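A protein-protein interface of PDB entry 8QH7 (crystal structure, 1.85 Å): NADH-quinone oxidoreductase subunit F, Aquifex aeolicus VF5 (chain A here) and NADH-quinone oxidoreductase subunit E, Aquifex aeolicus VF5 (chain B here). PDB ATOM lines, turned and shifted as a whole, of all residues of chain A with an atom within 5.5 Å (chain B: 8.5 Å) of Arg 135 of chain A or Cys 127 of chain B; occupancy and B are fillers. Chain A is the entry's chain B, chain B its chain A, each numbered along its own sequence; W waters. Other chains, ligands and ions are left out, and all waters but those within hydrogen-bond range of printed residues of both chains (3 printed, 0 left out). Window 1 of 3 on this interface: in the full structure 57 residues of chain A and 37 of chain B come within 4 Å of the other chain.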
ATOM      1  N   ALA A  93     -23.959 -24.494  25.375  1.00  0.00           N
ATOM      2  CA  ALA A  93     -23.014 -23.402  25.559  1.00  0.00           C
ATOM      3  C   ALA A  93     -22.730 -22.742  24.204  1.00  0.00           C
ATOM      4  O   ALA A  93     -21.608 -22.313  23.917  1.00  0.00           O
ATOM      5  CB  ALA A  93     -21.767 -23.946  26.224  1.00  0.00           C
ATOM      6  N   ASP A  94     -23.757 -22.647  23.345  1.00  0.00           N
ATOM      7  CA  ASP A  94     -23.553 -22.074  22.024  1.00  0.00           C
ATOM      8  C   ASP A  94     -23.632 -20.540  22.054  1.00  0.00           C
ATOM      9  O   ASP A  94     -23.243 -19.917  21.072  1.00  0.00           O
ATOM     10  CB  ASP A  94     -24.525 -22.601  20.969  1.00  0.00           C
ATOM     11  CG  ASP A  94     -23.992 -22.364  19.569  1.00  0.00           C
ATOM     12  OD1 ASP A  94     -22.919 -22.900  19.274  1.00  0.00           O
ATOM     13  OD2 ASP A  94     -24.627 -21.598  18.797  1.00  0.00           O
ATOM     14  N   GLU A  95     -24.129 -19.972  23.165  1.00  0.00           N
ATOM     15  CA  GLU A  95     -24.338 -18.545  23.399  1.00  0.00           C
ATOM     16  C   GLU A  95     -23.838 -17.661  22.250  1.00  0.00           C
ATOM     17  O   GLU A  95     -22.656 -17.325  22.191  1.00  0.00           O
ATOM     18  CB  GLU A  95     -23.651 -18.147  24.711  1.00  0.00           C
ATOM     19  CG  GLU A  95     -23.757 -16.659  25.025  1.00  0.00           C
ATOM     20  CD  GLU A  95     -23.227 -16.306  26.403  1.00  0.00           C
ATOM     21  OE1 GLU A  95     -22.000 -16.441  26.602  1.00  0.00           O
ATOM     22  OE2 GLU A  95     -24.059 -15.937  27.278  1.00  0.00           O
ATOM     23  N   SER A  96     -24.758 -17.246  21.363  1.00  0.00           N
ATOM     24  CA  SER A  96     -24.400 -16.458  20.192  1.00  0.00           C
ATOM     25  C   SER A  96     -25.380 -15.311  19.931  1.00  0.00           C
ATOM     26  O   SER A  96     -25.211 -14.611  18.935  1.00  0.00           O
ATOM     27  CB  SER A  96     -24.295 -17.344  18.966  1.00  0.00           C
ATOM     28  OG  SER A  96     -23.174 -18.208  19.072  1.00  0.00           O
ATOM     29  N   GLU A  97     -26.386 -15.127  20.802  1.00  0.00           N
ATOM     30  CA  GLU A  97     -27.316 -14.008  20.697  1.00  0.00           C
ATOM     31  C   GLU A  97     -26.553 -12.696  20.843  1.00  0.00           C
ATOM     32  O   GLU A  97     -25.758 -12.542  21.780  1.00  0.00           O
ATOM     33  CB  GLU A  97     -28.376 -14.092  21.798  1.00  0.00           C
ATOM     34  CG  GLU A  97     -29.487 -13.060  21.705  1.00  0.00           C
ATOM     35  CD  GLU A  97     -30.521 -13.301  20.616  1.00  0.00           C
ATOM     36  OE1 GLU A  97     -30.255 -14.135  19.722  1.00  0.00           O
ATOM     37  OE2 GLU A  97     -31.602 -12.661  20.680  1.00  0.00           O
ATOM     38  N   PRO A  98     -26.784 -11.696  19.962  1.00  0.00           N
ATOM     39  CA  PRO A  98     -26.184 -10.374  20.150  1.00  0.00           C
ATOM     40  C   PRO A  98     -26.369  -9.850  21.573  1.00  0.00           C
ATOM     41  O   PRO A  98     -27.443  -9.993  22.158  1.00  0.00           O
ATOM     42  CB  PRO A  98     -26.896  -9.508  19.104  1.00  0.00           C
ATOM     43  CG  PRO A  98     -27.184 -10.485  17.997  1.00  0.00           C
ATOM     44  CD  PRO A  98     -27.555 -11.773  18.708  1.00  0.00           C
ATOM     45  N   GLY A  99     -25.289  -9.273  22.120  1.00  0.00           N
ATOM     46  CA  GLY A  99     -25.292  -8.673  23.450  1.00  0.00           C
ATOM     47  C   GLY A  99     -25.172  -9.683  24.589  1.00  0.00           C
ATOM     48  O   GLY A  99     -25.193  -9.287  25.763  1.00  0.00           O
ATOM     49  N   THR A 100     -25.102 -10.980  24.250  1.00  0.00           N
ATOM     50  CA  THR A 100     -25.206 -12.024  25.261  1.00  0.00           C
ATOM     51  C   THR A 100     -23.837 -12.657  25.540  1.00  0.00           C
ATOM     52  O   THR A 100     -23.242 -13.291  24.667  1.00  0.00           O
ATOM     53  CB  THR A 100     -26.271 -13.049  24.863  1.00  0.00           C
ATOM     54  OG1 THR A 100     -27.420 -12.336  24.402  1.00  0.00           O
ATOM     55  CG2 THR A 100     -26.650 -13.952  26.015  1.00  0.00           C
ATOM     56  N   TYR A 133     -21.955 -28.528  24.287  1.00  0.00           N
ATOM     57  CA  TYR A 133     -21.751 -28.012  22.941  1.00  0.00           C
ATOM     58  C   TYR A 133     -21.396 -26.537  23.077  1.00  0.00           C
ATOM     59  O   TYR A 133     -22.250 -25.749  23.455  1.00  0.00           O
ATOM     60  CB  TYR A 133     -22.992 -28.238  22.080  1.00  0.00           C
ATOM     61  CG  TYR A 133     -22.819 -27.902  20.619  1.00  0.00           C
ATOM     62  CD1 TYR A 133     -22.930 -26.598  20.162  1.00  0.00           C
ATOM     63  CD2 TYR A 133     -22.549 -28.891  19.683  1.00  0.00           C
ATOM     64  CE1 TYR A 133     -22.784 -26.288  18.815  1.00  0.00           C
ATOM     65  CE2 TYR A 133     -22.403 -28.598  18.333  1.00  0.00           C
ATOM     66  CZ  TYR A 133     -22.524 -27.290  17.894  1.00  0.00           C
ATOM     67  OH  TYR A 133     -22.369 -26.995  16.549  1.00  0.00           O
ATOM     68  N   ILE A 134     -20.127 -26.198  22.855  1.00  0.00           N
ATOM     69  CA  ILE A 134     -19.672 -24.825  23.022  1.00  0.00           C
ATOM     70  C   ILE A 134     -19.369 -24.239  21.650  1.00  0.00           C
ATOM     71  O   ILE A 134     -18.751 -24.886  20.806  1.00  0.00           O
ATOM     72  CB  ILE A 134     -18.480 -24.718  24.005  1.00  0.00           C
ATOM     73  CG1 ILE A 134     -18.119 -23.254  24.300  1.00  0.00           C
ATOM     74  CG2 ILE A 134     -17.263 -25.488  23.525  1.00  0.00           C
ATOM     75  CD1 ILE A 134     -17.121 -23.089  25.432  1.00  0.00           C
ATOM     76  N   ARG A 135     -19.776 -22.983  21.435  1.00  0.00           N
ATOM     77  CA  ARG A 135     -19.575 -22.364  20.137  1.00  0.00           C
ATOM     78  C   ARG A 135     -18.083 -22.363  19.816  1.00  0.00           C
ATOM     79  O   ARG A 135     -17.242 -22.236  20.713  1.00  0.00           O
ATOM     80  CB  ARG A 135     -20.155 -20.945  20.122  1.00  0.00           C
ATOM     81  CG  ARG A 135     -19.505 -20.000  21.129  1.00  0.00           C
ATOM     82  CD  ARG A 135     -20.088 -18.604  21.076  1.00  0.00           C
ATOM     83  NE  ARG A 135     -19.948 -17.962  19.774  1.00  0.00           N
ATOM     84  CZ  ARG A 135     -20.288 -16.697  19.521  1.00  0.00           C
ATOM     85  NH1 ARG A 135     -20.824 -15.951  20.469  1.00  0.00           N
ATOM     86  NH2 ARG A 135     -20.101 -16.185  18.316  1.00  0.00           N
ATOM     87  N   GLY A 136     -17.773 -22.462  18.518  1.00  0.00           N
ATOM     88  CA  GLY A 136     -16.404 -22.469  18.032  1.00  0.00           C
ATOM     89  C   GLY A 136     -15.622 -21.197  18.374  1.00  0.00           C
ATOM     90  O   GLY A 136     -14.398 -21.241  18.463  1.00  0.00           O
ATOM     91  N   GLU A 137     -16.325 -20.072  18.539  1.00  0.00           N
ATOM     92  CA  GLU A 137     -15.680 -18.786  18.789  1.00  0.00           C
ATOM     93  C   GLU A 137     -15.369 -18.590  20.279  1.00  0.00           C
ATOM     94  O   GLU A 137     -14.950 -17.503  20.687  1.00  0.00           O
ATOM     95  CB  GLU A 137     -16.551 -17.639  18.273  1.00  0.00           C
ATOM     96  CG  GLU A 137     -16.889 -17.724  16.792  1.00  0.00           C
ATOM     97  CD  GLU A 137     -18.138 -18.523  16.450  1.00  0.00           C
ATOM     98  OE1 GLU A 137     -18.744 -19.163  17.382  1.00  0.00           O
ATOM     99  OE2 GLU A 137     -18.553 -18.461  15.265  1.00  0.00           O
ATOM    100  N   TYR A 138     -15.560 -19.645  21.086  1.00  0.00           N
ATOM    101  CA  TYR A 138     -15.119 -19.672  22.471  1.00  0.00           C
ATOM    102  C   TYR A 138     -14.024 -20.725  22.627  1.00  0.00           C
ATOM    103  O   TYR A 138     -14.208 -21.712  23.339  1.00  0.00           O
ATOM    104  CB  TYR A 138     -16.286 -20.004  23.407  1.00  0.00           C
ATOM    105  CG  TYR A 138     -17.321 -18.939  23.676  1.00  0.00           C
ATOM    106  CD1 TYR A 138     -17.145 -17.607  23.324  1.00  0.00           C
ATOM    107  CD2 TYR A 138     -18.479 -19.275  24.352  1.00  0.00           C
ATOM    108  CE1 TYR A 138     -18.110 -16.651  23.610  1.00  0.00           C
ATOM    109  CE2 TYR A 138     -19.443 -18.339  24.666  1.00  0.00           C
ATOM    110  CZ  TYR A 138     -19.252 -17.016  24.294  1.00  0.00           C
ATOM    111  OH  TYR A 138     -20.233 -16.121  24.592  1.00  0.00           O
ATOM    112  N   PRO A 139     -12.860 -20.579  21.958  1.00  0.00           N
ATOM    113  CA  PRO A 139     -11.800 -21.584  22.053  1.00  0.00           C
ATOM    114  C   PRO A 139     -11.232 -21.728  23.462  1.00  0.00           C
ATOM    115  O   PRO A 139     -10.946 -22.840  23.906  1.00  0.00           O
ATOM    116  CB  PRO A 139     -10.756 -21.118  21.028  1.00  0.00           C
ATOM    117  CG  PRO A 139     -11.020 -19.629  20.861  1.00  0.00           C
ATOM    118  CD  PRO A 139     -12.509 -19.476  21.053  1.00  0.00           C
ATOM    119  N   ARG A 175     -17.447 -28.799  19.803  1.00  0.00           N
ATOM    120  CA  ARG A 175     -17.283 -27.414  19.391  1.00  0.00           C
ATOM    121  C   ARG A 175     -18.157 -27.143  18.171  1.00  0.00           C
ATOM    122  O   ARG A 175     -18.207 -27.957  17.247  1.00  0.00           O
ATOM    123  CB  ARG A 175     -15.825 -27.121  19.030  1.00  0.00           C
ATOM    124  CG  ARG A 175     -14.863 -27.149  20.203  1.00  0.00           C
ATOM    125  CD  ARG A 175     -13.474 -26.744  19.759  1.00  0.00           C
ATOM    126  NE  ARG A 175     -13.406 -25.327  19.428  1.00  0.00           N
ATOM    127  CZ  ARG A 175     -12.390 -24.753  18.804  1.00  0.00           C
ATOM    128  NH1 ARG A 175     -11.374 -25.482  18.378  1.00  0.00           N
ATOM    129  NH2 ARG A 175     -12.414 -23.451  18.586  1.00  0.00           N
ATOM    130  N   GLY A 176     -18.843 -25.999  18.207  1.00  0.00           N
ATOM    131  CA  GLY A 176     -19.461 -25.391  17.039  1.00  0.00           C
ATOM    132  C   GLY A 176     -18.416 -24.898  16.040  1.00  0.00           C
ATOM    133  O   GLY A 176     -17.212 -25.019  16.270  1.00  0.00           O
ATOM    134  N   ALA A 177     -18.888 -24.380  14.905  1.00  0.00           N
ATOM    135  CA  ALA A 177     -17.990 -23.894  13.871  1.00  0.00           C
ATOM    136  C   ALA A 177     -18.629 -22.764  13.066  1.00  0.00           C
ATOM    137  O   ALA A 177     -18.359 -22.653  11.876  1.00  0.00           O
ATOM    138  CB  ALA A 177     -17.579 -25.037  12.984  1.00  0.00           C
ATOM    139  N   PHE A 341     -27.973  -9.606  10.918  1.00  0.00           N
ATOM    140  CA  PHE A 341     -27.731 -10.773  11.744  1.00  0.00           C
ATOM    141  C   PHE A 341     -28.580 -11.952  11.260  1.00  0.00           C
ATOM    142  O   PHE A 341     -28.056 -13.044  11.037  1.00  0.00           O
ATOM    143  CB  PHE A 341     -28.019 -10.467  13.212  1.00  0.00           C
ATOM    144  CG  PHE A 341     -27.723 -11.629  14.114  1.00  0.00           C
ATOM    145  CD1 PHE A 341     -26.415 -11.919  14.469  1.00  0.00           C
ATOM    146  CD2 PHE A 341     -28.741 -12.443  14.583  1.00  0.00           C
ATOM    147  CE1 PHE A 341     -26.132 -13.004  15.285  1.00  0.00           C
ATOM    148  CE2 PHE A 341     -28.453 -13.525  15.401  1.00  0.00           C
ATOM    149  CZ  PHE A 341     -27.149 -13.805  15.740  1.00  0.00           C
ATOM    150  N   HIS B  35     -11.589 -28.225  12.408  1.00  0.00           N
ATOM    151  CA  HIS B  35     -10.838 -27.222  13.153  1.00  0.00           C
ATOM    152  C   HIS B  35      -9.341 -27.547  13.135  1.00  0.00           C
ATOM    153  O   HIS B  35      -8.505 -26.673  12.913  1.00  0.00           O
ATOM    154  CB  HIS B  35     -11.353 -27.115  14.594  1.00  0.00           C
ATOM    155  CG  HIS B  35     -12.585 -26.296  14.759  1.00  0.00           C
ATOM    156  ND1 HIS B  35     -12.643 -24.963  14.421  1.00  0.00           N
ATOM    157  CD2 HIS B  35     -13.792 -26.605  15.271  1.00  0.00           C
ATOM    158  CE1 HIS B  35     -13.850 -24.497  14.720  1.00  0.00           C
ATOM    159  NE2 HIS B  35     -14.562 -25.477  15.232  1.00  0.00           N
ATOM    160  N   MET B  72     -16.985 -20.817  10.054  1.00  0.00           N
ATOM    161  CA  MET B  72     -15.616 -20.669  10.535  1.00  0.00           C
ATOM    162  C   MET B  72     -14.620 -21.274   9.543  1.00  0.00           C
ATOM    163  O   MET B  72     -13.477 -20.818   9.474  1.00  0.00           O
ATOM    164  CB  MET B  72     -15.419 -21.300  11.918  1.00  0.00           C
ATOM    165  CG  MET B  72     -15.964 -20.433  13.034  1.00  0.00           C
ATOM    166  SD  MET B  72     -15.572 -21.032  14.703  1.00  0.00           S
ATOM    167  CE  MET B  72     -13.831 -20.629  14.805  1.00  0.00           C
ATOM    168  N   VAL B  85     -13.285  -9.783  13.059  1.00  0.00           N
ATOM    169  CA  VAL B  85     -13.786  -8.495  13.504  1.00  0.00           C
ATOM    170  C   VAL B  85     -15.308  -8.588  13.610  1.00  0.00           C
ATOM    171  O   VAL B  85     -15.996  -8.896  12.639  1.00  0.00           O
ATOM    172  CB  VAL B  85     -13.354  -7.365  12.554  1.00  0.00           C
ATOM    173  CG1 VAL B  85     -13.991  -6.039  12.945  1.00  0.00           C
ATOM    174  CG2 VAL B  85     -11.840  -7.244  12.452  1.00  0.00           C
ATOM    175  N   CYS B  86     -15.839  -8.314  14.804  1.00  0.00           N
ATOM    176  CA  CYS B  86     -17.276  -8.363  15.002  1.00  0.00           C
ATOM    177  C   CYS B  86     -17.956  -7.160  14.340  1.00  0.00           C
ATOM    178  O   CYS B  86     -17.575  -6.014  14.582  1.00  0.00           O
ATOM    179  CB  CYS B  86     -17.620  -8.406  16.480  1.00  0.00           C
ATOM    180  SG  CYS B  86     -19.404  -8.397  16.747  1.00  0.00           S
ATOM    181  N   VAL B  87     -18.993  -7.432  13.540  1.00  0.00           N
ATOM    182  CA  VAL B  87     -19.704  -6.398  12.800  1.00  0.00           C
ATOM    183  C   VAL B  87     -21.163  -6.310  13.256  1.00  0.00           C
ATOM    184  O   VAL B  87     -21.968  -5.659  12.589  1.00  0.00           O
ATOM    185  CB  VAL B  87     -19.631  -6.629  11.271  1.00  0.00           C
ATOM    186  CG1 VAL B  87     -18.193  -6.545  10.772  1.00  0.00           C
ATOM    187  CG2 VAL B  87     -20.284  -7.938  10.827  1.00  0.00           C
ATOM    188  N   SER B  88     -21.508  -6.951  14.382  1.00  0.00           N
ATOM    189  CA  SER B  88     -22.879  -6.972  14.873  1.00  0.00           C
ATOM    190  C   SER B  88     -23.176  -5.708  15.677  1.00  0.00           C
ATOM    191  O   SER B  88     -22.297  -4.869  15.868  1.00  0.00           O
ATOM    192  CB  SER B  88     -23.161  -8.214  15.676  1.00  0.00           C
ATOM    193  OG  SER B  88     -23.186  -9.358  14.840  1.00  0.00           O
ATOM    194  N   ILE B  89     -24.416  -5.627  16.189  1.00  0.00           N
ATOM    195  CA  ILE B  89     -25.017  -4.388  16.681  1.00  0.00           C
ATOM    196  C   ILE B  89     -24.137  -3.678  17.722  1.00  0.00           C
ATOM    197  O   ILE B  89     -23.874  -2.485  17.570  1.00  0.00           O
ATOM    198  CB  ILE B  89     -26.470  -4.627  17.162  1.00  0.00           C
ATOM    199  CG1 ILE B  89     -27.124  -3.382  17.769  1.00  0.00           C
ATOM    200  CG2 ILE B  89     -26.587  -5.814  18.103  1.00  0.00           C
ATOM    201  CD1 ILE B  89     -27.403  -2.305  16.785  1.00  0.00           C
ATOM    202  N   VAL B  90     -23.688  -4.347  18.791  1.00  0.00           N
ATOM    203  CA  VAL B  90     -23.016  -3.615  19.866  1.00  0.00           C
ATOM    204  C   VAL B  90     -21.667  -3.073  19.385  1.00  0.00           C
ATOM    205  O   VAL B  90     -21.359  -1.899  19.591  1.00  0.00           O
ATOM    206  CB  VAL B  90     -22.852  -4.447  21.149  1.00  0.00           C
ATOM    207  CG1 VAL B  90     -22.423  -3.567  22.320  1.00  0.00           C
ATOM    208  CG2 VAL B  90     -24.126  -5.207  21.496  1.00  0.00           C
ATOM    209  N   CYS B  91     -20.855  -3.919  18.749  1.00  0.00           N
ATOM    210  CA  CYS B  91     -19.562  -3.472  18.259  1.00  0.00           C
ATOM    211  C   CYS B  91     -19.740  -2.363  17.222  1.00  0.00           C
ATOM    212  O   CYS B  91     -18.948  -1.425  17.208  1.00  0.00           O
ATOM    213  CB  CYS B  91     -18.741  -4.645  17.744  1.00  0.00           C
ATOM    214  SG  CYS B  91     -18.273  -5.778  19.085  1.00  0.00           S
ATOM    215  N   PRO B 124     -14.886 -10.675   8.696  1.00  0.00           N
ATOM    216  CA  PRO B 124     -16.034 -10.089   9.387  1.00  0.00           C
ATOM    217  C   PRO B 124     -16.905 -11.198   9.980  1.00  0.00           C
ATOM    218  O   PRO B 124     -17.214 -12.173   9.297  1.00  0.00           O
ATOM    219  CB  PRO B 124     -16.721  -9.285   8.278  1.00  0.00           C
ATOM    220  CG  PRO B 124     -16.406 -10.058   7.009  1.00  0.00           C
ATOM    221  CD  PRO B 124     -15.037 -10.662   7.233  1.00  0.00           C
ATOM    222  N   VAL B 125     -17.243 -11.081  11.274  1.00  0.00           N
ATOM    223  CA  VAL B 125     -18.002 -12.116  11.958  1.00  0.00           C
ATOM    224  C   VAL B 125     -19.158 -11.471  12.710  1.00  0.00           C
ATOM    225  O   VAL B 125     -19.132 -10.277  13.013  1.00  0.00           O
ATOM    226  CB  VAL B 125     -17.137 -12.951  12.927  1.00  0.00           C
ATOM    227  CG1 VAL B 125     -15.992 -13.651  12.205  1.00  0.00           C
ATOM    228  CG2 VAL B 125     -16.610 -12.118  14.090  1.00  0.00           C
ATOM    229  N   GLN B 126     -20.130 -12.317  13.064  1.00  0.00           N
ATOM    230  CA  GLN B 126     -21.253 -11.923  13.897  1.00  0.00           C
ATOM    231  C   GLN B 126     -20.825 -11.935  15.369  1.00  0.00           C
ATOM    232  O   GLN B 126     -19.750 -12.428  15.697  1.00  0.00           O
ATOM    233  CB  GLN B 126     -22.435 -12.856  13.643  1.00  0.00           C
ATOM    234  CG  GLN B 126     -22.776 -13.025  12.165  1.00  0.00           C
ATOM    235  CD  GLN B 126     -23.196 -11.728  11.525  1.00  0.00           C
ATOM    236  OE1 GLN B 126     -24.198 -11.142  11.912  1.00  0.00           O
ATOM    237  NE2 GLN B 126     -22.468 -11.299  10.505  1.00  0.00           N
ATOM    238  N   CYS B 127     -21.702 -11.393  16.230  1.00  0.00           N
ATOM    239  CA  CYS B 127     -21.473 -11.198  17.660  1.00  0.00           C
ATOM    240  C   CYS B 127     -20.643 -12.324  18.265  1.00  0.00           C
ATOM    241  O   CYS B 127     -21.045 -13.492  18.216  1.00  0.00           O
ATOM    242  CB  CYS B 127     -22.782 -11.150  18.437  1.00  0.00           C
ATOM    243  SG  CYS B 127     -22.540 -10.888  20.217  1.00  0.00           S
ATOM    244  N   LEU B 128     -19.516 -11.937  18.873  1.00  0.00           N
ATOM    245  CA  LEU B 128     -18.547 -12.859  19.469  1.00  0.00           C
ATOM    246  C   LEU B 128     -18.795 -13.090  20.965  1.00  0.00           C
ATOM    247  O   LEU B 128     -17.979 -13.736  21.638  1.00  0.00           O
ATOM    248  CB  LEU B 128     -17.151 -12.263  19.256  1.00  0.00           C
ATOM    249  CG  LEU B 128     -16.602 -12.355  17.834  1.00  0.00           C
ATOM    250  CD1 LEU B 128     -15.334 -11.525  17.700  1.00  0.00           C
ATOM    251  CD2 LEU B 128     -16.328 -13.806  17.457  1.00  0.00           C
ATOM    252  N   GLY B 129     -19.906 -12.572  21.496  1.00  0.00           N
ATOM    253  CA  GLY B 129     -20.223 -12.770  22.901  1.00  0.00           C
ATOM    254  C   GLY B 129     -19.189 -12.141  23.836  1.00  0.00           C
ATOM    255  O   GLY B 129     -18.837 -12.735  24.852  1.00  0.00           O
ATOM    256  N   ALA B 130     -18.736 -10.917  23.519  1.00  0.00           N
ATOM    257  CA  ALA B 130     -17.937 -10.120  24.444  1.00  0.00           C
ATOM    258  C   ALA B 130     -18.323  -8.641  24.342  1.00  0.00           C
ATOM    259  O   ALA B 130     -17.467  -7.768  24.459  1.00  0.00           O
ATOM    260  CB  ALA B 130     -16.454 -10.317  24.184  1.00  0.00           C
ATOM    261  N   CYS B 131     -19.637  -8.384  24.255  1.00  0.00           N
ATOM    262  CA  CYS B 131     -20.176  -7.120  23.778  1.00  0.00           C
ATOM    263  C   CYS B 131     -19.861  -5.964  24.735  1.00  0.00           C
ATOM    264  O   CYS B 131     -19.803  -4.812  24.307  1.00  0.00           O
ATOM    265  CB  CYS B 131     -21.682  -7.248  23.566  1.00  0.00           C
ATOM    266  SG  CYS B 131     -22.174  -8.816  22.798  1.00  0.00           S
ATOM    267  N   SER B 132     -19.663  -6.261  26.030  1.00  0.00           N
ATOM    268  CA  SER B 132     -19.293  -5.247  27.019  1.00  0.00           C
ATOM    269  C   SER B 132     -17.902  -4.672  26.738  1.00  0.00           C
ATOM    270  O   SER B 132     -17.559  -3.587  27.216  1.00  0.00           O
ATOM    271  CB  SER B 132     -19.387  -5.797  28.435  1.00  0.00           C
ATOM    272  OG  SER B 132     -18.552  -6.936  28.589  1.00  0.00           O
ATOM    273  N   VAL B 136     -14.927  -5.718  19.510  1.00  0.00           N
ATOM    274  CA  VAL B 136     -14.196  -6.953  19.765  1.00  0.00           C
ATOM    275  C   VAL B 136     -13.552  -7.478  18.478  1.00  0.00           C
ATOM    276  O   VAL B 136     -14.169  -7.440  17.402  1.00  0.00           O
ATOM    277  CB  VAL B 136     -15.137  -8.028  20.345  1.00  0.00           C
ATOM    278  CG1 VAL B 136     -14.396  -9.323  20.639  1.00  0.00           C
ATOM    279  CG2 VAL B 136     -15.870  -7.547  21.589  1.00  0.00           C
ATOM    280  N   MET B 138     -10.797 -11.043  17.296  1.00  0.00           N
ATOM    281  CA  MET B 138      -9.952 -12.173  17.637  1.00  0.00           C
ATOM    282  C   MET B 138      -8.745 -12.183  16.703  1.00  0.00           C
ATOM    283  O   MET B 138      -8.826 -11.710  15.575  1.00  0.00           O
ATOM    284  CB  MET B 138     -10.705 -13.498  17.497  1.00  0.00           C
ATOM    285  CG  MET B 138     -11.929 -13.596  18.385  1.00  0.00           C
ATOM    286  SD  MET B 138     -12.760 -15.197  18.233  1.00  0.00           S
ATOM    287  CE  MET B 138     -11.646 -16.198  19.217  1.00  0.00           C
ATOM    288  N   GLU B 143      -8.594 -13.190  21.892  1.00  0.00           N
ATOM    289  CA  GLU B 143      -9.681 -12.234  21.736  1.00  0.00           C
ATOM    290  C   GLU B 143      -9.421 -10.979  22.560  1.00  0.00           C
ATOM    291  O   GLU B 143      -8.970 -11.071  23.704  1.00  0.00           O
ATOM    292  CB  GLU B 143     -10.995 -12.866  22.180  1.00  0.00           C
ATOM    293  CG  GLU B 143     -12.191 -11.956  21.990  1.00  0.00           C
ATOM    294  CD  GLU B 143     -13.506 -12.704  22.046  1.00  0.00           C
ATOM    295  OE1 GLU B 143     -14.100 -12.761  23.142  1.00  0.00           O
ATOM    296  OE2 GLU B 143     -13.905 -13.273  21.002  1.00  0.00           O
HETATM  297  O   HOH W   1     -19.242 -15.138  15.551  1.00  0.00           O
HETATM  298  O   HOH W   2     -22.936 -13.847  21.683  1.00  0.00           O
HETATM  299  O   HOH W   3     -23.391 -14.424  17.010  1.00  0.00           O
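The backbone carbonyl oxygen (O) of Gly 176 of chain A lies within hydrogen-bond range of a ring nitrogen (NE2) of His 35 of chain B (2.9 Å). The side-chain sulfur (SG) of Cys 131 of chain B sits close to the backbone NH (N) of Gly 99 of chain A (3.2 Å). The backbone NH (N) of Gly 99 of chain A sits close to the side-chain sulfur (SG) of Cys 127 of chain B (3.7 Å). N of Met 72 of chain B sits at hydrogen-bond distance from O of Ala 177 of chain A, at 2.9 Å. O of Cys 127 of chain B sits at hydrogen-bond distance from NH2 of Arg 135 of chain A.
OG of Ser 96 of chain A lies close to NE of Arg 135 of chain A (3.3 Å). N of Gly 136 of chain A sits close to O of Gly 176 of chain A (3.5 Å). The side-chain carboxylate (OE1) of Glu 95 of chain A is in hydrogen-bond range of the side-chain hydroxyl (OH) of Tyr 138 of chain A. NH1 of Arg 135 of chain A lies within hydrogen-bond range of O of Glu 95 of chain A.
Among the printed residues, pairs that only touch across the chains: Phe 341 of chain A with Gln 126 of chain B (3.5 Å), Tyr 138 of chain A with Leu 128 of chain B (3.5 Å), Thr 100 of chain A with Gly 129 of chain B (3.5 Å), Arg 135 of chain A with Leu 128 of chain B (3.5 Å), Arg 135 of chain A with Gly 129 of chain B (3.6 Å), Tyr 138 of chain A with Gly 129 of chain B (3.7 Å), Gly 136 of chain A with Met 72 of chain B (3.7 Å), Pro 98 of chain A with Cys 127 of chain B (3.7 Å), Ala 177 of chain A with His 35 of chain B (3.8 Å), Pro 98 of chain A with Ile 89 of chain B (3.8 Å), Glu 137 of chain A with Met 138 of chain B (3.8 Å), Pro 139 of chain A with Met 138 of chain B (3.9 Å), Arg 175 of chain A with His 35 of chain B (3.9 Å), Thr 100 of chain A with Cys 131 of chain B (3.9 Å), Glu 137 of chain A with Leu 128 of chain B (3.9 Å), Glu 97 of chain A with Cys 127 of chain B (3.9 Å) and Glu 137 of chain A with Met 72 of chain B (3.9 Å).
Of the printed residues of chain B, Thr 100 of chain A touches Gly 129 and Cys 131. Gly 136 of chain A touches one residue of chain B. Of chain B, only Leu 128 (3.5 Å) and Gly 129 (3.7 Å) come within 4 Å of Tyr 138 of chain A. Of the printed residues of chain B, Pro 139 of chain A touches Met 138 (3.9 Å). Of the printed residues of chain B, Phe 341 of chain A touches Gln 126. Of the printed residues of chain A, His 35 of chain B touches Arg 175, Gly 176 and Ala 177. Cys 127 of chain B touches just these residues of chain A: Glu 97, Pro 98, Gly 99 and Arg 135. Of the printed residues of chain A, Leu 128 of chain B touches Arg 135 (3.5 Å), Glu 137 (3.9 Å) and Tyr 138 (3.5 Å). The nearest printed residue of chain A that does not touch Leu 128 of chain B is Thr 100 of chain A (5.8 Å).
Hydrophobic or aromatic side chains of chain A within 4 Å of the printed part of chain B: Pro 98, Tyr 138, Pro 139, Ala 177 and Phe 341. Along chain A the printed residues that touch a printed residue of chain B span positions 97 to 341. Hydrophobic or aromatic side chains of chain B within 4 Å of the printed part of chain A: His 35, Met 72, Ile 89, Leu 128 and Met 138. Along chain B the printed residues that touch a printed residue of chain A span positions 35 to 138. Among the printed residues, 22 pairs touch across the chains. Among the printed residues, no Asp or Glu carboxylate lies within 4 Å of a Lys or Arg side-chain nitrogen of the other chain.
Water W3 lies within hydrogen-bond range of the backbone carbonyl oxygen (O) of Ser 96 of chain A (2.7 Å) and the backbone carbonyl oxygen (O) of Cys 127 of chain B (2.8 Å). Water W1 lies within hydrogen-bond range of O of Gln 126 of chain B (2.8 Å), NH2 of Arg 135 of chain A (3.1 Å) and OE2 of Glu 137 of chain A (3.4 Å).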
